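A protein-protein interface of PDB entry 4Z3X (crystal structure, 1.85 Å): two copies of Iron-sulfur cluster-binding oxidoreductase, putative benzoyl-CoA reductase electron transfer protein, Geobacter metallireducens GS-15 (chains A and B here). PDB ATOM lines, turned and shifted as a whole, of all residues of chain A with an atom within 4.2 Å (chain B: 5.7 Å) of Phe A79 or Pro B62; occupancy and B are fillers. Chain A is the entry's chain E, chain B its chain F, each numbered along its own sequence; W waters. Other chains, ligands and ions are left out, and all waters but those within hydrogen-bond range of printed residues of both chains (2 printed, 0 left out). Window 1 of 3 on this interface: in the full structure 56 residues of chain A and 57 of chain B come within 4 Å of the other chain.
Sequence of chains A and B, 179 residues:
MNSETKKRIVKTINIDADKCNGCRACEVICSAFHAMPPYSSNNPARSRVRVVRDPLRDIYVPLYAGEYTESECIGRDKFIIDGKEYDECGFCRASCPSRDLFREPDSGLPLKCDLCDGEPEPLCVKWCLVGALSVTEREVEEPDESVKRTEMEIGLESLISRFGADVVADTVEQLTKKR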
ATOM      1  N   ASP A  77     -27.368 -16.267 -12.676  1.00  0.00           N
ATOM      2  CA  ASP A  77     -27.720 -16.754 -11.333  1.00  0.00           C
ATOM      3  C   ASP A  77     -26.702 -16.204 -10.290  1.00  0.00           C
ATOM      4  O   ASP A  77     -25.559 -15.972 -10.635  1.00  0.00           O
ATOM      5  CB  ASP A  77     -27.760 -18.286 -11.308  1.00  0.00           C
ATOM      6  CG  ASP A  77     -26.403 -18.965 -11.709  1.00  0.00           C
ATOM      7  OD1 ASP A  77     -25.492 -18.316 -12.251  1.00  0.00           O
ATOM      8  OD2 ASP A  77     -26.255 -20.188 -11.470  1.00  0.00           O
ATOM      9  N   LYS A  78     -27.138 -16.009  -9.041  1.00  0.00           N
ATOM     10  CA  LYS A  78     -26.268 -15.533  -7.970  1.00  0.00           C
ATOM     11  C   LYS A  78     -26.681 -16.215  -6.681  1.00  0.00           C
ATOM     12  O   LYS A  78     -27.831 -16.070  -6.232  1.00  0.00           O
ATOM     13  CB  LYS A  78     -26.377 -14.001  -7.821  1.00  0.00           C
ATOM     14  CG  LYS A  78     -25.343 -13.351  -6.842  1.00  0.00           C
ATOM     15  CD  LYS A  78     -25.532 -11.808  -6.862  1.00  0.00           C
ATOM     16  CE  LYS A  78     -24.354 -11.111  -6.207  1.00  0.00           C
ATOM     17  NZ  LYS A  78     -24.549 -11.132  -4.747  1.00  0.00           N
ATOM     18  N   PHE A  79     -25.767 -17.010  -6.123  1.00  0.00           N
ATOM     19  CA  PHE A  79     -26.053 -17.859  -4.964  1.00  0.00           C
ATOM     20  C   PHE A  79     -25.638 -17.287  -3.601  1.00  0.00           C
ATOM     21  O   PHE A  79     -24.574 -16.631  -3.457  1.00  0.00           O
ATOM     22  CB  PHE A  79     -25.320 -19.182  -5.126  1.00  0.00           C
ATOM     23  CG  PHE A  79     -25.889 -20.089  -6.143  1.00  0.00           C
ATOM     24  CD1 PHE A  79     -27.116 -20.740  -5.922  1.00  0.00           C
ATOM     25  CD2 PHE A  79     -25.174 -20.380  -7.296  1.00  0.00           C
ATOM     26  CE1 PHE A  79     -27.654 -21.608  -6.855  1.00  0.00           C
ATOM     27  CE2 PHE A  79     -25.716 -21.267  -8.221  1.00  0.00           C
ATOM     28  CZ  PHE A  79     -26.972 -21.882  -7.999  1.00  0.00           C
ATOM     29  N   ILE A  80     -26.476 -17.547  -2.602  1.00  0.00           N
ATOM     30  CA  ILE A  80     -26.048 -17.553  -1.204  1.00  0.00           C
ATOM     31  C   ILE A  80     -26.089 -19.013  -0.777  1.00  0.00           C
ATOM     32  O   ILE A  80     -27.147 -19.673  -0.885  1.00  0.00           O
ATOM     33  CB  ILE A  80     -26.964 -16.718  -0.304  1.00  0.00           C
ATOM     34  CG1 ILE A  80     -27.033 -15.251  -0.796  1.00  0.00           C
ATOM     35  CG2 ILE A  80     -26.554 -16.863   1.125  1.00  0.00           C
ATOM     36  CD1 ILE A  80     -27.932 -14.407   0.072  1.00  0.00           C
ATOM     37  N   ILE A  81     -24.943 -19.504  -0.302  1.00  0.00           N
ATOM     38  CA  ILE A  81     -24.776 -20.881   0.158  1.00  0.00           C
ATOM     39  C   ILE A  81     -23.945 -20.915   1.445  1.00  0.00           C
ATOM     40  O   ILE A  81     -22.805 -20.411   1.454  1.00  0.00           O
ATOM     41  CB  ILE A  81     -24.046 -21.743  -0.881  1.00  0.00           C
ATOM     42  CG1 ILE A  81     -24.752 -21.661  -2.255  1.00  0.00           C
ATOM     43  CG2 ILE A  81     -23.984 -23.201  -0.340  1.00  0.00           C
ATOM     44  CD1 ILE A  81     -23.942 -22.257  -3.427  1.00  0.00           C
ATOM     45  N   LYS A  84     -22.309 -17.626   2.516  1.00  0.00           N
ATOM     46  CA  LYS A  84     -21.411 -16.917   1.654  1.00  0.00           C
ATOM     47  C   LYS A  84     -22.249 -16.366   0.507  1.00  0.00           C
ATOM     48  O   LYS A  84     -22.959 -17.122  -0.137  1.00  0.00           O
ATOM     49  CB  LYS A  84     -20.305 -17.840   1.143  1.00  0.00           C
ATOM     50  CG  LYS A  84     -19.263 -18.244   2.214  1.00  0.00           C
ATOM     51  CD  LYS A  84     -18.204 -19.160   1.614  1.00  0.00           C
ATOM     52  CE  LYS A  84     -17.021 -19.213   2.580  1.00  0.00           C
ATOM     53  NZ  LYS A  84     -16.069 -20.316   2.352  1.00  0.00           N
ATOM     54  N   GLU A  85     -22.216 -15.054   0.299  1.00  0.00           N
ATOM     55  CA  GLU A  85     -22.738 -14.480  -0.943  1.00  0.00           C
ATOM     56  C   GLU A  85     -21.735 -14.539  -2.114  1.00  0.00           C
ATOM     57  O   GLU A  85     -20.814 -13.723  -2.215  1.00  0.00           O
ATOM     58  CB  GLU A  85     -23.127 -13.034  -0.697  1.00  0.00           C
ATOM     59  CG  GLU A  85     -23.707 -12.833   0.680  1.00  0.00           C
ATOM     60  CD  GLU A  85     -24.616 -11.628   0.777  1.00  0.00           C
ATOM     61  OE1 GLU A  85     -25.050 -11.105  -0.283  1.00  0.00           O
ATOM     62  OE2 GLU A  85     -24.924 -11.230   1.923  1.00  0.00           O
ATOM     63  N   TYR A  86     -21.938 -15.475  -3.021  1.00  0.00           N
ATOM     64  CA  TYR A  86     -21.050 -15.622  -4.178  1.00  0.00           C
ATOM     65  C   TYR A  86     -21.346 -14.581  -5.257  1.00  0.00           C
ATOM     66  O   TYR A  86     -22.338 -13.830  -5.160  1.00  0.00           O
ATOM     67  CB  TYR A  86     -21.170 -17.032  -4.713  1.00  0.00           C
ATOM     68  CG  TYR A  86     -20.549 -18.081  -3.793  1.00  0.00           C
ATOM     69  CD1 TYR A  86     -19.197 -18.352  -3.865  1.00  0.00           C
ATOM     70  CD2 TYR A  86     -21.338 -18.840  -2.857  1.00  0.00           C
ATOM     71  CE1 TYR A  86     -18.608 -19.290  -3.055  1.00  0.00           C
ATOM     72  CE2 TYR A  86     -20.760 -19.818  -2.066  1.00  0.00           C
ATOM     73  CZ  TYR A  86     -19.384 -20.015  -2.163  1.00  0.00           C
ATOM     74  OH  TYR A  86     -18.760 -20.952  -1.425  1.00  0.00           O
ATOM     75  N   ILE B  13     -30.926 -13.818 -11.230  1.00  0.00           N
ATOM     76  CA  ILE B  13     -31.735 -14.753 -10.431  1.00  0.00           C
ATOM     77  C   ILE B  13     -31.001 -14.998  -9.136  1.00  0.00           C
ATOM     78  O   ILE B  13     -29.935 -15.615  -9.115  1.00  0.00           O
ATOM     79  CB  ILE B  13     -31.943 -16.084 -11.136  1.00  0.00           C
ATOM     80  CG1 ILE B  13     -32.496 -15.924 -12.553  1.00  0.00           C
ATOM     81  CG2 ILE B  13     -32.887 -17.018 -10.314  1.00  0.00           C
ATOM     82  CD1 ILE B  13     -32.128 -17.114 -13.472  1.00  0.00           C
ATOM     83  N   ILE B  15     -30.541 -16.590  -5.566  1.00  0.00           N
ATOM     84  CA  ILE B  15     -30.954 -17.889  -5.019  1.00  0.00           C
ATOM     85  C   ILE B  15     -30.335 -17.998  -3.662  1.00  0.00           C
ATOM     86  O   ILE B  15     -29.103 -18.155  -3.513  1.00  0.00           O
ATOM     87  CB  ILE B  15     -30.551 -19.080  -5.951  1.00  0.00           C
ATOM     88  CG1 ILE B  15     -31.123 -18.835  -7.359  1.00  0.00           C
ATOM     89  CG2 ILE B  15     -31.051 -20.440  -5.360  1.00  0.00           C
ATOM     90  CD1 ILE B  15     -30.421 -19.549  -8.550  1.00  0.00           C
ATOM     91  N   ASP B  16     -31.176 -17.834  -2.653  1.00  0.00           N
ATOM     92  CA  ASP B  16     -30.707 -18.052  -1.340  1.00  0.00           C
ATOM     93  C   ASP B  16     -30.810 -19.549  -0.970  1.00  0.00           C
ATOM     94  O   ASP B  16     -31.768 -19.963  -0.331  1.00  0.00           O
ATOM     95  CB  ASP B  16     -31.511 -17.205  -0.362  1.00  0.00           C
ATOM     96  CG  ASP B  16     -30.888 -17.164   1.034  1.00  0.00           C
ATOM     97  OD1 ASP B  16     -30.245 -18.149   1.454  1.00  0.00           O
ATOM     98  OD2 ASP B  16     -31.049 -16.120   1.708  1.00  0.00           O
ATOM     99  N   ALA B  17     -29.813 -20.351  -1.340  1.00  0.00           N
ATOM    100  CA  ALA B  17     -29.869 -21.784  -1.033  1.00  0.00           C
ATOM    101  C   ALA B  17     -30.008 -22.115   0.478  1.00  0.00           C
ATOM    102  O   ALA B  17     -30.339 -23.262   0.853  1.00  0.00           O
ATOM    103  CB  ALA B  17     -28.634 -22.512  -1.676  1.00  0.00           C
ATOM    104  N   CYS B  20     -33.845 -22.612   1.124  1.00  0.00           N
ATOM    105  CA  CYS B  20     -34.489 -23.656   0.360  1.00  0.00           C
ATOM    106  C   CYS B  20     -34.858 -24.845   1.241  1.00  0.00           C
ATOM    107  O   CYS B  20     -34.104 -25.197   2.169  1.00  0.00           O
ATOM    108  CB  CYS B  20     -33.563 -24.073  -0.793  1.00  0.00           C
ATOM    109  SG  CYS B  20     -34.389 -25.300  -1.859  1.00  0.00           S
ATOM    110  N   CYS B  26     -41.005 -25.475  -7.410  1.00  0.00           N
ATOM    111  CA  CYS B  26     -40.504 -24.673  -8.492  1.00  0.00           C
ATOM    112  C   CYS B  26     -40.408 -25.537  -9.730  1.00  0.00           C
ATOM    113  O   CYS B  26     -40.804 -25.122 -10.837  1.00  0.00           O
ATOM    114  CB  CYS B  26     -39.120 -24.045  -8.165  1.00  0.00           C
ATOM    115  SG  CYS B  26     -37.926 -25.248  -7.389  1.00  0.00           S
ATOM    116  N   VAL B  49     -35.838 -25.141 -14.057  1.00  0.00           N
ATOM    117  CA  VAL B  49     -35.168 -25.011 -12.767  1.00  0.00           C
ATOM    118  C   VAL B  49     -35.169 -26.437 -12.150  1.00  0.00           C
ATOM    119  O   VAL B  49     -36.167 -27.119 -12.132  1.00  0.00           O
ATOM    120  CB  VAL B  49     -35.844 -23.988 -11.815  1.00  0.00           C
ATOM    121  CG1 VAL B  49     -37.257 -24.438 -11.481  1.00  0.00           C
ATOM    122  CG2 VAL B  49     -35.015 -23.774 -10.564  1.00  0.00           C
ATOM    123  N   ARG B  50     -34.013 -26.884 -11.697  1.00  0.00           N
ATOM    124  CA  ARG B  50     -33.841 -28.240 -11.205  1.00  0.00           C
ATOM    125  C   ARG B  50     -33.046 -28.149  -9.900  1.00  0.00           C
ATOM    126  O   ARG B  50     -31.996 -27.494  -9.846  1.00  0.00           O
ATOM    127  CB  ARG B  50     -33.119 -29.080 -12.250  1.00  0.00           C
ATOM    128  CG  ARG B  50     -33.941 -29.458 -13.507  1.00  0.00           C
ATOM    129  CD  ARG B  50     -35.248 -30.290 -13.242  1.00  0.00           C
ATOM    130  NE  ARG B  50     -34.982 -31.614 -12.685  1.00  0.00           N
ATOM    131  CZ  ARG B  50     -34.529 -32.631 -13.400  1.00  0.00           C
ATOM    132  NH1 ARG B  50     -34.361 -32.488 -14.705  1.00  0.00           N
ATOM    133  NH2 ARG B  50     -34.303 -33.822 -12.807  1.00  0.00           N
ATOM    134  N   VAL B  51     -33.581 -28.731  -8.842  1.00  0.00           N
ATOM    135  CA  VAL B  51     -32.986 -28.622  -7.533  1.00  0.00           C
ATOM    136  C   VAL B  51     -32.050 -29.776  -7.205  1.00  0.00           C
ATOM    137  O   VAL B  51     -32.460 -30.951  -7.230  1.00  0.00           O
ATOM    138  CB  VAL B  51     -34.038 -28.575  -6.459  1.00  0.00           C
ATOM    139  CG1 VAL B  51     -33.412 -28.237  -5.137  1.00  0.00           C
ATOM    140  CG2 VAL B  51     -35.094 -27.553  -6.827  1.00  0.00           C
ATOM    141  N   VAL B  52     -30.774 -29.447  -6.940  1.00  0.00           N
ATOM    142  CA  VAL B  52     -29.901 -30.437  -6.372  1.00  0.00           C
ATOM    143  C   VAL B  52     -30.359 -30.647  -4.932  1.00  0.00           C
ATOM    144  O   VAL B  52     -30.347 -29.717  -4.137  1.00  0.00           O
ATOM    145  CB  VAL B  52     -28.419 -30.033  -6.360  1.00  0.00           C
ATOM    146  CG1 VAL B  52     -27.635 -31.181  -5.716  1.00  0.00           C
ATOM    147  CG2 VAL B  52     -27.926 -29.806  -7.744  1.00  0.00           C
ATOM    148  N   TYR B  60     -29.135 -28.275  -0.820  1.00  0.00           N
ATOM    149  CA  TYR B  60     -30.405 -27.831  -1.453  1.00  0.00           C
ATOM    150  C   TYR B  60     -30.136 -26.672  -2.358  1.00  0.00           C
ATOM    151  O   TYR B  60     -30.140 -25.510  -1.929  1.00  0.00           O
ATOM    152  CB  TYR B  60     -31.433 -27.403  -0.417  1.00  0.00           C
ATOM    153  CG  TYR B  60     -31.687 -28.452   0.617  1.00  0.00           C
ATOM    154  CD1 TYR B  60     -30.845 -28.573   1.733  1.00  0.00           C
ATOM    155  CD2 TYR B  60     -32.766 -29.331   0.486  1.00  0.00           C
ATOM    156  CE1 TYR B  60     -31.105 -29.546   2.702  1.00  0.00           C
ATOM    157  CE2 TYR B  60     -33.026 -30.302   1.426  1.00  0.00           C
ATOM    158  CZ  TYR B  60     -32.197 -30.421   2.517  1.00  0.00           C
ATOM    159  OH  TYR B  60     -32.480 -31.393   3.444  1.00  0.00           O
ATOM    160  N   VAL B  61     -29.894 -26.973  -3.622  1.00  0.00           N
ATOM    161  CA  VAL B  61     -29.434 -25.941  -4.503  1.00  0.00           C
ATOM    162  C   VAL B  61     -30.262 -25.850  -5.815  1.00  0.00           C
ATOM    163  O   VAL B  61     -30.043 -26.630  -6.730  1.00  0.00           O
ATOM    164  CB  VAL B  61     -27.982 -26.142  -4.883  1.00  0.00           C
ATOM    165  CG1 VAL B  61     -27.580 -24.961  -5.666  1.00  0.00           C
ATOM    166  CG2 VAL B  61     -27.068 -26.283  -3.630  1.00  0.00           C
ATOM    167  N   PRO B  62     -31.157 -24.849  -5.924  1.00  0.00           N
ATOM    168  CA  PRO B  62     -31.880 -24.640  -7.201  1.00  0.00           C
ATOM    169  C   PRO B  62     -30.931 -24.222  -8.338  1.00  0.00           C
ATOM    170  O   PRO B  62     -30.210 -23.233  -8.175  1.00  0.00           O
ATOM    171  CB  PRO B  62     -32.868 -23.516  -6.874  1.00  0.00           C
ATOM    172  CG  PRO B  62     -33.023 -23.531  -5.346  1.00  0.00           C
ATOM    173  CD  PRO B  62     -31.648 -23.970  -4.838  1.00  0.00           C
ATOM    174  N   LEU B  63     -30.872 -25.000  -9.418  1.00  0.00           N
ATOM    175  CA  LEU B  63     -30.098 -24.672 -10.607  1.00  0.00           C
ATOM    176  C   LEU B  63     -30.988 -24.286 -11.782  1.00  0.00           C
ATOM    177  O   LEU B  63     -31.869 -25.042 -12.182  1.00  0.00           O
ATOM    178  CB  LEU B  63     -29.228 -25.815 -11.052  1.00  0.00           C
ATOM    179  CG  LEU B  63     -27.738 -25.857 -10.874  1.00  0.00           C
ATOM    180  CD1 LEU B  63     -27.235 -26.936 -11.785  1.00  0.00           C
ATOM    181  CD2 LEU B  63     -27.098 -24.481 -11.188  1.00  0.00           C
ATOM    182  N   TYR B  64     -30.747 -23.113 -12.354  1.00  0.00           N
ATOM    183  CA  TYR B  64     -31.494 -22.698 -13.540  1.00  0.00           C
ATOM    184  C   TYR B  64     -30.817 -23.067 -14.864  1.00  0.00           C
ATOM    185  O   TYR B  64     -29.631 -22.930 -14.996  1.00  0.00           O
ATOM    186  CB  TYR B  64     -31.702 -21.230 -13.469  1.00  0.00           C
ATOM    187  CG  TYR B  64     -32.771 -20.868 -12.496  1.00  0.00           C
ATOM    188  CD1 TYR B  64     -32.566 -20.987 -11.142  1.00  0.00           C
ATOM    189  CD2 TYR B  64     -34.005 -20.396 -12.951  1.00  0.00           C
ATOM    190  CE1 TYR B  64     -33.551 -20.609 -10.236  1.00  0.00           C
ATOM    191  CE2 TYR B  64     -34.995 -20.005 -12.051  1.00  0.00           C
ATOM    192  CZ  TYR B  64     -34.776 -20.132 -10.705  1.00  0.00           C
ATOM    193  OH  TYR B  64     -35.772 -19.767  -9.811  1.00  0.00           O
ATOM    194  N   PHE B  91     -22.704 -27.359 -10.415  1.00  0.00           N
ATOM    195  CA  PHE B  91     -23.218 -26.022 -10.519  1.00  0.00           C
ATOM    196  C   PHE B  91     -23.417 -25.592 -11.983  1.00  0.00           C
ATOM    197  O   PHE B  91     -23.687 -24.438 -12.242  1.00  0.00           O
ATOM    198  CB  PHE B  91     -22.242 -25.054  -9.779  1.00  0.00           C
ATOM    199  CG  PHE B  91     -22.189 -25.302  -8.316  1.00  0.00           C
ATOM    200  CD1 PHE B  91     -23.131 -24.710  -7.464  1.00  0.00           C
ATOM    201  CD2 PHE B  91     -21.226 -26.151  -7.780  1.00  0.00           C
ATOM    202  CE1 PHE B  91     -23.095 -24.989  -6.109  1.00  0.00           C
ATOM    203  CE2 PHE B  91     -21.189 -26.414  -6.423  1.00  0.00           C
ATOM    204  CZ  PHE B  91     -22.120 -25.805  -5.588  1.00  0.00           C
ATOM    205  N   ALA B 132     -36.993 -18.207  -1.236  1.00  0.00           N
ATOM    206  CA  ALA B 132     -35.590 -18.516  -1.543  1.00  0.00           C
ATOM    207  C   ALA B 132     -35.165 -17.889  -2.879  1.00  0.00           C
ATOM    208  O   ALA B 132     -33.972 -17.773  -3.157  1.00  0.00           O
ATOM    209  CB  ALA B 132     -35.379 -20.032  -1.560  1.00  0.00           C
ATOM    210  N   LEU B 133     -36.133 -17.519  -3.734  1.00  0.00           N
ATOM    211  CA  LEU B 133     -35.815 -17.092  -5.113  1.00  0.00           C
ATOM    212  C   LEU B 133     -36.321 -15.696  -5.313  1.00  0.00           C
ATOM    213  O   LEU B 133     -37.327 -15.321  -4.705  1.00  0.00           O
ATOM    214  CB  LEU B 133     -36.449 -18.021  -6.151  1.00  0.00           C
ATOM    215  CG  LEU B 133     -36.417 -19.513  -5.907  1.00  0.00           C
ATOM    216  CD1 LEU B 133     -37.283 -20.251  -6.986  1.00  0.00           C
ATOM    217  CD2 LEU B 133     -35.031 -19.952  -6.041  1.00  0.00           C
HETATM  218  O   HOH W   1     -23.917 -22.013 -11.942  1.00  0.00           O
HETATM  219  O   HOH W   2     -28.815 -21.299 -11.220  1.00  0.00           O
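Water W1 bridges the backbone carbonyl oxygen (O) of Phe B91 and the side-chain carboxylate (OD2) of Asp A77. Water W2 lies within hydrogen-bond range of OD2 of Asp A77 (2.8 Å) and N of Tyr B64 (2.9 Å).
Of chain B, only Ile B15 (3.4 Å), Val B61 (3.6 Å) and Pro B62 (3.3 Å) come within 4 Å of Phe A79. Printed residues of chain B within 4 Å of Asp A77: Ile B13 (3.3 Å). Of the printed residues of chain A, Asp B16 touches Ile A80. Of the printed residues of chain A, Val B61 touches Phe A79 (3.6 Å). Of the printed residues of chain B, Ile A80 touches Ile B15, Asp B16 and Ala B17. Of the printed residues of chain B, Lys A78 touches Ile B13 (2.8 Å) and Ile B15 (2.8 Å). The nearest printed residue of chain B that does not touch Asp A77 is Ile B15 (4.04 Å).
No position is printed for both chains. Of the 10 pairs that touch across the chains among the printed residues, none has its exchanged pair printed and touching as well.
The backbone carbonyl oxygen (O) of Lys A78 lies within hydrogen-bond range of the backbone NH (N) of Ile B15. The backbone carbonyl oxygen (O) of Ile B15 sits at hydrogen-bond distance from the backbone NH (N) of Ile A80, at 2.8 Å. N of Lys A78 sits at hydrogen-bond distance from O of Ile B13 (2.8 Å). O of Ile A80 sits at hydrogen-bond distance from N of Ala B17 (2.8 Å).
Asp A77 touches Ile B13 (CA to O, 3.3 Å). Ile B15 touches Phe A79. CE1 of Phe A79 touches CG1 of Val B61, at 3.6 Å. Phe A79 touches Pro B62 (CE1 to O, 3.3 Å). Ile A80 touches Asp B16. Ile A81 touches Phe B91.
Hydrophobic or aromatic side chains of chain B that line the printed part of chain A: Ile B15, Ala B17, Val B61 and Phe B91. Of the 8 printed residues of chain A, 5 touch a printed residue of chain B. Printed residues of chain A that touch a printed residue of chain B: Asp A77, Lys A78, Phe A79, Ile A80 and Ile A81. Hydrophobic or aromatic side chains of chain A within 4 Å of the printed part of chain B: Phe A79, Ile A80 and Ile A81. Among the printed residues, 10 pairs touch across the chains. Among the printed residues, no Asp or Glu carboxylate lies within 4 Å of a Lys or Arg side-chain nitrogen of the other chain.
The backbone NH (N) of Tyr A86 sits at hydrogen-bond distance from the backbone carbonyl oxygen (O) of Phe A79. N of Asp B16 is in hydrogen-bond range of O of Ala B132 (2.8 Å). O of Val B52 is in hydrogen-bond range of N of Val B61 (2.8 Å).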
